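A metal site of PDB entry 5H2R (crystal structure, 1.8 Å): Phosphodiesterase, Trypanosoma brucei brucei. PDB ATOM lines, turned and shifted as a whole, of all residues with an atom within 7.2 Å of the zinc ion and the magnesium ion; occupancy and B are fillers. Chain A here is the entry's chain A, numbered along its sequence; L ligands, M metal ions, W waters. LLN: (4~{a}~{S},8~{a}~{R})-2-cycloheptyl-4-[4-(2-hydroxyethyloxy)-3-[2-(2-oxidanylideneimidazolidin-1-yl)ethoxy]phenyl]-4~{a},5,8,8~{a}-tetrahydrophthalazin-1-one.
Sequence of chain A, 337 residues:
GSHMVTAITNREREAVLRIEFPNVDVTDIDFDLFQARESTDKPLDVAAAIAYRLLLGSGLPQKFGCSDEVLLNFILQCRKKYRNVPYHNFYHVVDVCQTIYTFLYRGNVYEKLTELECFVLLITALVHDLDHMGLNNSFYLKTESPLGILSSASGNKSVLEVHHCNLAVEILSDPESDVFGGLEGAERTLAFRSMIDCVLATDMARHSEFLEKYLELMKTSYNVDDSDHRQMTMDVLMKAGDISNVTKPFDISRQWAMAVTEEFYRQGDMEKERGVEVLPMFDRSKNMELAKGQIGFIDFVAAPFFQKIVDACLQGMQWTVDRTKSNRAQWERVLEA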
ATOM      1  N   TYR A  87      24.924  -9.159 -22.245  1.00  0.00           N
ATOM      2  CA  TYR A  87      23.725 -10.026 -22.286  1.00  0.00           C
ATOM      3  C   TYR A  87      23.317 -10.635 -20.938  1.00  0.00           C
ATOM      4  O   TYR A  87      22.190 -10.425 -20.516  1.00  0.00           O
ATOM      5  CB  TYR A  87      23.894 -11.128 -23.339  1.00  0.00           C
ATOM      6  CG  TYR A  87      22.638 -11.954 -23.507  1.00  0.00           C
ATOM      7  CD1 TYR A  87      21.588 -11.503 -24.313  1.00  0.00           C
ATOM      8  CD2 TYR A  87      22.427 -13.104 -22.737  1.00  0.00           C
ATOM      9  CE1 TYR A  87      20.413 -12.241 -24.437  1.00  0.00           C
ATOM     10  CE2 TYR A  87      21.243 -13.827 -22.837  1.00  0.00           C
ATOM     11  CZ  TYR A  87      20.237 -13.398 -23.682  1.00  0.00           C
ATOM     12  OH  TYR A  87      19.077 -14.123 -23.753  1.00  0.00           O
ATOM     13  N   HIS A  88      24.208 -11.429 -20.292  1.00  0.00           N
ATOM     14  CA  HIS A  88      23.880 -12.080 -19.020  1.00  0.00           C
ATOM     15  C   HIS A  88      23.935 -11.129 -17.787  1.00  0.00           C
ATOM     16  O   HIS A  88      24.619 -11.393 -16.788  1.00  0.00           O
ATOM     17  CB  HIS A  88      24.747 -13.322 -18.838  1.00  0.00           C
ATOM     18  CG  HIS A  88      24.368 -14.454 -19.735  1.00  0.00           C
ATOM     19  ND1 HIS A  88      25.156 -14.812 -20.801  1.00  0.00           N
ATOM     20  CD2 HIS A  88      23.300 -15.287 -19.670  1.00  0.00           C
ATOM     21  CE1 HIS A  88      24.544 -15.838 -21.364  1.00  0.00           C
ATOM     22  NE2 HIS A  88      23.439 -16.163 -20.716  1.00  0.00           N
ATOM     23  N   HIS A  92      18.353  -9.618 -18.385  1.00  0.00           N
ATOM     24  CA  HIS A  92      18.115 -10.937 -18.942  1.00  0.00           C
ATOM     25  C   HIS A  92      17.221 -11.765 -18.006  1.00  0.00           C
ATOM     26  O   HIS A  92      16.250 -12.351 -18.473  1.00  0.00           O
ATOM     27  CB  HIS A  92      19.446 -11.678 -19.153  1.00  0.00           C
ATOM     28  CG  HIS A  92      19.263 -13.118 -19.473  1.00  0.00           C
ATOM     29  ND1 HIS A  92      18.481 -13.523 -20.542  1.00  0.00           N
ATOM     30  CD2 HIS A  92      19.708 -14.208 -18.799  1.00  0.00           C
ATOM     31  CE1 HIS A  92      18.497 -14.847 -20.528  1.00  0.00           C
ATOM     32  NE2 HIS A  92      19.199 -15.303 -19.474  1.00  0.00           N
ATOM     33  N   VAL A  93      17.544 -11.799 -16.690  1.00  0.00           N
ATOM     34  CA  VAL A  93      16.765 -12.619 -15.747  1.00  0.00           C
ATOM     35  C   VAL A  93      15.394 -12.003 -15.493  1.00  0.00           C
ATOM     36  O   VAL A  93      14.422 -12.753 -15.318  1.00  0.00           O
ATOM     37  CB  VAL A  93      17.512 -13.040 -14.450  1.00  0.00           C
ATOM     38  CG1 VAL A  93      18.771 -13.817 -14.812  1.00  0.00           C
ATOM     39  CG2 VAL A  93      17.846 -11.853 -13.554  1.00  0.00           C
ATOM     40  N   VAL A  96      13.495 -13.089 -18.541  1.00  0.00           N
ATOM     41  CA  VAL A  96      13.128 -14.508 -18.449  1.00  0.00           C
ATOM     42  C   VAL A  96      11.922 -14.704 -17.504  1.00  0.00           C
ATOM     43  O   VAL A  96      10.999 -15.454 -17.834  1.00  0.00           O
ATOM     44  CB  VAL A  96      14.351 -15.416 -18.111  1.00  0.00           C
ATOM     45  CG1 VAL A  96      13.919 -16.835 -17.780  1.00  0.00           C
ATOM     46  CG2 VAL A  96      15.345 -15.427 -19.273  1.00  0.00           C
ATOM     47  N   ALA A 125      13.703 -18.121 -12.278  1.00  0.00           N
ATOM     48  CA  ALA A 125      14.104 -17.268 -13.394  1.00  0.00           C
ATOM     49  C   ALA A 125      15.056 -16.184 -12.920  1.00  0.00           C
ATOM     50  O   ALA A 125      16.009 -15.886 -13.601  1.00  0.00           O
ATOM     51  CB  ALA A 125      12.877 -16.623 -14.059  1.00  0.00           C
ATOM     52  N   HIS A 128      18.628 -17.911 -12.032  1.00  0.00           N
ATOM     53  CA  HIS A 128      19.145 -18.891 -12.976  1.00  0.00           C
ATOM     54  C   HIS A 128      20.519 -18.550 -13.620  1.00  0.00           C
ATOM     55  O   HIS A 128      21.117 -19.469 -14.144  1.00  0.00           O
ATOM     56  CB  HIS A 128      18.103 -19.287 -14.035  1.00  0.00           C
ATOM     57  CG  HIS A 128      18.148 -18.490 -15.288  1.00  0.00           C
ATOM     58  ND1 HIS A 128      17.443 -17.307 -15.396  1.00  0.00           N
ATOM     59  CD2 HIS A 128      18.796 -18.726 -16.454  1.00  0.00           C
ATOM     60  CE1 HIS A 128      17.663 -16.880 -16.634  1.00  0.00           C
ATOM     61  NE2 HIS A 128      18.475 -17.695 -17.302  1.00  0.00           N
ATOM     62  N   ASP A 129      20.991 -17.278 -13.581  1.00  0.00           N
ATOM     63  CA  ASP A 129      22.301 -16.879 -14.120  1.00  0.00           C
ATOM     64  C   ASP A 129      23.158 -16.091 -13.158  1.00  0.00           C
ATOM     65  O   ASP A 129      24.031 -15.360 -13.635  1.00  0.00           O
ATOM     66  CB  ASP A 129      22.140 -16.111 -15.453  1.00  0.00           C
ATOM     67  CG  ASP A 129      21.930 -17.011 -16.656  1.00  0.00           C
ATOM     68  OD1 ASP A 129      22.510 -18.115 -16.668  1.00  0.00           O
ATOM     69  OD2 ASP A 129      21.221 -16.578 -17.612  1.00  0.00           O
ATOM     70  N   LEU A 130      22.957 -16.254 -11.818  1.00  0.00           N
ATOM     71  CA  LEU A 130      23.688 -15.487 -10.807  1.00  0.00           C
ATOM     72  C   LEU A 130      25.187 -15.490 -11.024  1.00  0.00           C
ATOM     73  O   LEU A 130      25.770 -16.541 -11.211  1.00  0.00           O
ATOM     74  CB  LEU A 130      23.354 -15.921  -9.368  1.00  0.00           C
ATOM     75  CG  LEU A 130      21.928 -15.599  -8.896  1.00  0.00           C
ATOM     76  CD1 LEU A 130      21.541 -16.496  -7.751  1.00  0.00           C
ATOM     77  CD2 LEU A 130      21.777 -14.104  -8.478  1.00  0.00           C
ATOM     78  N   HIS A 132      27.061 -14.493 -13.577  1.00  0.00           N
ATOM     79  CA  HIS A 132      27.540 -14.823 -14.913  1.00  0.00           C
ATOM     80  C   HIS A 132      28.529 -13.693 -15.279  1.00  0.00           C
ATOM     81  O   HIS A 132      28.240 -12.523 -14.979  1.00  0.00           O
ATOM     82  CB  HIS A 132      26.374 -14.873 -15.909  1.00  0.00           C
ATOM     83  CG  HIS A 132      26.646 -15.701 -17.135  1.00  0.00           C
ATOM     84  ND1 HIS A 132      27.494 -15.242 -18.135  1.00  0.00           N
ATOM     85  CD2 HIS A 132      26.125 -16.887 -17.509  1.00  0.00           C
ATOM     86  CE1 HIS A 132      27.494 -16.197 -19.055  1.00  0.00           C
ATOM     87  NE2 HIS A 132      26.670 -17.196 -18.728  1.00  0.00           N
ATOM     88  N   LEU A 160      28.891 -23.251 -14.851  1.00  0.00           N
ATOM     89  CA  LEU A 160      28.183 -22.051 -14.408  1.00  0.00           C
ATOM     90  C   LEU A 160      26.894 -22.381 -13.671  1.00  0.00           C
ATOM     91  O   LEU A 160      26.568 -21.673 -12.751  1.00  0.00           O
ATOM     92  CB  LEU A 160      27.868 -21.148 -15.596  1.00  0.00           C
ATOM     93  CG  LEU A 160      29.041 -20.403 -16.228  1.00  0.00           C
ATOM     94  CD1 LEU A 160      28.624 -19.832 -17.550  1.00  0.00           C
ATOM     95  CD2 LEU A 160      29.531 -19.286 -15.324  1.00  0.00           C
ATOM     96  N   GLU A 161      26.142 -23.356 -14.171  1.00  0.00           N
ATOM     97  CA  GLU A 161      24.827 -23.731 -13.603  1.00  0.00           C
ATOM     98  C   GLU A 161      24.913 -24.194 -12.150  1.00  0.00           C
ATOM     99  O   GLU A 161      24.074 -23.797 -11.350  1.00  0.00           O
ATOM    100  CB  GLU A 161      24.123 -24.745 -14.487  1.00  0.00           C
ATOM    101  CG  GLU A 161      23.693 -24.207 -15.850  1.00  0.00           C
ATOM    102  CD  GLU A 161      24.796 -24.070 -16.877  1.00  0.00           C
ATOM    103  OE1 GLU A 161      25.856 -24.711 -16.735  1.00  0.00           O
ATOM    104  OE2 GLU A 161      24.585 -23.321 -17.852  1.00  0.00           O
ATOM    105  N   HIS A 164      25.534 -21.072 -10.254  1.00  0.00           N
ATOM    106  CA  HIS A 164      24.269 -20.316 -10.126  1.00  0.00           C
ATOM    107  C   HIS A 164      23.422 -20.833  -8.968  1.00  0.00           C
ATOM    108  O   HIS A 164      22.891 -20.042  -8.203  1.00  0.00           O
ATOM    109  CB  HIS A 164      23.469 -20.313 -11.454  1.00  0.00           C
ATOM    110  CG  HIS A 164      24.213 -19.778 -12.656  1.00  0.00           C
ATOM    111  ND1 HIS A 164      25.038 -18.668 -12.569  1.00  0.00           N
ATOM    112  CD2 HIS A 164      24.163 -20.180 -13.954  1.00  0.00           C
ATOM    113  CE1 HIS A 164      25.519 -18.471 -13.787  1.00  0.00           C
ATOM    114  NE2 HIS A 164      25.027 -19.355 -14.650  1.00  0.00           N
ATOM    115  N   VAL A 199      17.449 -24.828 -12.805  1.00  0.00           N
ATOM    116  CA  VAL A 199      18.708 -24.117 -13.116  1.00  0.00           C
ATOM    117  C   VAL A 199      19.679 -25.083 -13.806  1.00  0.00           C
ATOM    118  O   VAL A 199      20.265 -24.734 -14.823  1.00  0.00           O
ATOM    119  CB  VAL A 199      19.357 -23.404 -11.908  1.00  0.00           C
ATOM    120  CG1 VAL A 199      20.683 -22.737 -12.304  1.00  0.00           C
ATOM    121  CG2 VAL A 199      18.403 -22.371 -11.314  1.00  0.00           C
ATOM    122  N   THR A 202      19.237 -25.583 -17.526  1.00  0.00           N
ATOM    123  CA  THR A 202      19.534 -24.480 -18.462  1.00  0.00           C
ATOM    124  C   THR A 202      20.870 -24.626 -19.200  1.00  0.00           C
ATOM    125  O   THR A 202      21.179 -23.810 -20.078  1.00  0.00           O
ATOM    126  CB  THR A 202      19.419 -23.116 -17.796  1.00  0.00           C
ATOM    127  OG1 THR A 202      20.420 -23.040 -16.783  1.00  0.00           O
ATOM    128  CG2 THR A 202      18.000 -22.843 -17.258  1.00  0.00           C
ATOM    129  N   ASP A 203      21.679 -25.644 -18.821  1.00  0.00           N
ATOM    130  CA  ASP A 203      22.940 -25.895 -19.530  1.00  0.00           C
ATOM    131  C   ASP A 203      22.586 -26.409 -20.944  1.00  0.00           C
ATOM    132  O   ASP A 203      22.089 -27.531 -21.088  1.00  0.00           O
ATOM    133  CB  ASP A 203      23.820 -26.890 -18.765  1.00  0.00           C
ATOM    134  CG  ASP A 203      25.092 -27.251 -19.500  1.00  0.00           C
ATOM    135  OD1 ASP A 203      25.372 -26.631 -20.558  1.00  0.00           O
ATOM    136  OD2 ASP A 203      25.833 -28.116 -19.015  1.00  0.00           O
ATOM    137  N   MET A 204      22.883 -25.591 -21.978  1.00  0.00           N
ATOM    138  CA  MET A 204      22.569 -25.922 -23.384  1.00  0.00           C
ATOM    139  C   MET A 204      23.323 -27.125 -23.953  1.00  0.00           C
ATOM    140  O   MET A 204      22.879 -27.692 -24.957  1.00  0.00           O
ATOM    141  CB  MET A 204      22.702 -24.716 -24.315  1.00  0.00           C
ATOM    142  CG  MET A 204      21.648 -23.649 -24.099  1.00  0.00           C
ATOM    143  SD  MET A 204      19.931 -24.161 -24.381  1.00  0.00           S
ATOM    144  CE  MET A 204      19.885 -24.262 -26.148  1.00  0.00           C
ATOM    145  N   MET A 238      11.568 -23.215 -18.053  1.00  0.00           N
ATOM    146  CA  MET A 238      12.792 -22.477 -17.736  1.00  0.00           C
ATOM    147  C   MET A 238      13.634 -22.372 -19.023  1.00  0.00           C
ATOM    148  O   MET A 238      14.056 -21.269 -19.408  1.00  0.00           O
ATOM    149  CB  MET A 238      13.582 -23.213 -16.631  1.00  0.00           C
ATOM    150  CG  MET A 238      14.698 -22.382 -15.988  1.00  0.00           C
ATOM    151  SD  MET A 238      14.382 -20.687 -15.405  1.00  0.00           S
ATOM    152  CE  MET A 238      12.911 -20.896 -14.402  1.00  0.00           C
ATOM    153  N   GLY A 241      11.999 -20.045 -21.562  1.00  0.00           N
ATOM    154  CA  GLY A 241      12.227 -18.666 -21.160  1.00  0.00           C
ATOM    155  C   GLY A 241      13.635 -18.249 -21.582  1.00  0.00           C
ATOM    156  O   GLY A 241      13.824 -17.162 -22.141  1.00  0.00           O
ATOM    157  N   ASP A 242      14.624 -19.128 -21.363  1.00  0.00           N
ATOM    158  CA  ASP A 242      16.028 -18.862 -21.722  1.00  0.00           C
ATOM    159  C   ASP A 242      16.294 -18.613 -23.235  1.00  0.00           C
ATOM    160  O   ASP A 242      17.143 -17.783 -23.580  1.00  0.00           O
ATOM    161  CB  ASP A 242      16.923 -19.979 -21.200  1.00  0.00           C
ATOM    162  CG  ASP A 242      18.121 -19.515 -20.401  1.00  0.00           C
ATOM    163  OD1 ASP A 242      18.302 -18.290 -20.244  1.00  0.00           O
ATOM    164  OD2 ASP A 242      18.850 -20.386 -19.892  1.00  0.00           O
ATOM    165  N   ILE A 243      15.593 -19.340 -24.118  1.00  0.00           N
ATOM    166  CA  ILE A 243      15.747 -19.201 -25.582  1.00  0.00           C
ATOM    167  C   ILE A 243      14.530 -18.485 -26.205  1.00  0.00           C
ATOM    168  O   ILE A 243      14.268 -18.607 -27.406  1.00  0.00           O
ATOM    169  CB  ILE A 243      16.084 -20.561 -26.250  1.00  0.00           C
ATOM    170  CG1 ILE A 243      14.979 -21.627 -26.030  1.00  0.00           C
ATOM    171  CG2 ILE A 243      17.462 -21.069 -25.788  1.00  0.00           C
ATOM    172  CD1 ILE A 243      14.994 -22.815 -27.117  1.00  0.00           C
HETATM  173  C1  LLN L   1      19.214 -13.535 -28.932  1.00  0.00           C
HETATM  174  C2  LLN L   1      20.581 -15.520 -28.605  1.00  0.00           C
HETATM  175  C3  LLN L   1      20.283 -15.603 -27.246  1.00  0.00           C
HETATM  176  O1  LLN L   1      20.063 -14.571 -29.459  1.00  0.00           O
HETATM  177  O2  LLN L   1      21.807 -16.255 -30.486  1.00  0.00           O
HETATM  178  O3  LLN L   1      22.960 -13.889 -33.611  1.00  0.00           O
HETATM  179  C11 LLN L   1      26.105 -14.549 -32.204  1.00  0.00           C
HETATM  180  C12 LLN L   1      23.953 -14.350 -33.064  1.00  0.00           C
HETATM  181  C13 LLN L   1      22.328 -18.608 -26.197  1.00  0.00           C
HETATM  182  C14 LLN L   1      24.130 -21.589 -26.996  1.00  0.00           C
HETATM  183  C15 LLN L   1      22.929 -22.464 -27.531  1.00  0.00           C
HETATM  184  C16 LLN L   1      23.161 -23.500 -28.647  1.00  0.00           C
HETATM  185  C17 LLN L   1      23.357 -22.924 -30.038  1.00  0.00           C
HETATM  186  C18 LLN L   1      24.610 -22.112 -30.307  1.00  0.00           C
HETATM  187  C19 LLN L   1      24.806 -20.854 -29.459  1.00  0.00           C
HETATM  188  C20 LLN L   1      25.211 -21.100 -28.010  1.00  0.00           C
HETATM  189  C21 LLN L   1      23.762 -20.564 -24.769  1.00  0.00           C
HETATM  190  C22 LLN L   1      23.207 -19.357 -24.024  1.00  0.00           C
HETATM  191  C23 LLN L   1      22.910 -19.681 -22.549  1.00  0.00           C
HETATM  192  C24 LLN L   1      21.626 -20.443 -22.399  1.00  0.00           C
HETATM  193  C25 LLN L   1      20.624 -20.343 -23.262  1.00  0.00           C
HETATM  194  C26 LLN L   1      20.753 -19.717 -24.626  1.00  0.00           C
HETATM  195  C27 LLN L   1      21.958 -18.774 -24.735  1.00  0.00           C
HETATM  196  O4  LLN L   1      24.225 -21.541 -24.211  1.00  0.00           O
HETATM  197  N3  LLN L   1      23.670 -20.481 -26.135  1.00  0.00           N
HETATM  198  N2  LLN L   1      23.118 -19.415 -26.816  1.00  0.00           N
HETATM  199  C5  LLN L   1      21.739 -17.522 -27.026  1.00  0.00           C
HETATM  200  C4  LLN L   1      20.857 -16.594 -26.473  1.00  0.00           C
HETATM  201  C6  LLN L   1      22.036 -17.452 -28.381  1.00  0.00           C
HETATM  202  C7  LLN L   1      21.446 -16.475 -29.184  1.00  0.00           C
HETATM  203  C   LLN L   1      18.205 -13.102 -29.970  1.00  0.00           C
HETATM  204  O   LLN L   1      17.340 -14.161 -30.331  1.00  0.00           O
HETATM  205  C8  LLN L   1      22.679 -17.188 -31.138  1.00  0.00           C
HETATM  206  C9  LLN L   1      22.997 -16.633 -32.518  1.00  0.00           C
HETATM  207  N   LLN L   1      24.048 -15.601 -32.512  1.00  0.00           N
HETATM  208  N1  LLN L   1      25.127 -13.722 -32.888  1.00  0.00           N
HETATM  209  C10 LLN L   1      25.281 -15.743 -31.733  1.00  0.00           C
HETATM  210 ZN    ZN M   1      19.805 -17.324 -18.943  1.00  0.00          ZN
HETATM  211 MG    MG M   2      22.791 -19.692 -18.011  1.00  0.00          MG
HETATM  212  O   HOH W   1      23.622 -18.774 -19.605  1.00  0.00           O
HETATM  213  O   HOH W   2      22.804 -21.642 -18.901  1.00  0.00           O
HETATM  214  O   HOH W   3      21.018 -19.316 -18.895  1.00  0.00           O
HETATM  215  O   HOH W   4      20.999 -17.381 -20.832  1.00  0.00           O
HETATM  216  O   HOH W   5      21.870 -20.872 -16.301  1.00  0.00           O
HETATM  217  O   HOH W   6      24.549 -20.135 -17.264  1.00  0.00           O
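The side-chain carboxylate (OD1) of Asp 129 sits close to a ring nitrogen (NE2) of His 164, at 3.5 Å. A ring nitrogen (ND1) of His 128 sits at hydrogen-bond distance from the backbone carbonyl oxygen of Ala 125, at 2.7 Å. A ring nitrogen (ND1) of His 92 sits at hydrogen-bond distance from the side-chain hydroxyl (OH) of Tyr 87, at 3.3 Å.
Within 4 Å of the magnesium ion: Asp 129.
The zinc ion is bound by OD2 of Asp 129 (2.1 Å), NE2 of His 128 (2.1 Å), NE2 of His 92 (2.2 Å), OD1 of Asp 242 (2.2 Å), water W4 (2.2 Å) and water W3 (2.3 Å). The zinc ion has six donor atoms within binding distance.
The magnesium ion is bound by water W6, water W3, water W1, OD1 of Asp 129, water W2 and water W5. The magnesium ion has six donor atoms within binding distance.
Water W6 lies within hydrogen-bond range of a ring nitrogen (NE2) of His 164 and the side-chain carboxylate of Glu 161. Water W2 lies within hydrogen-bond range of the side-chain carboxylate (OE2) of Glu 161 and the backbone carbonyl oxygen (O) of Thr 202. Water W5 lies within hydrogen-bond range of the side-chain hydroxyl (OG1) of Thr 202 (2.7 Å) and the backbone carbonyl oxygen (O) of His 128 (2.7 Å).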
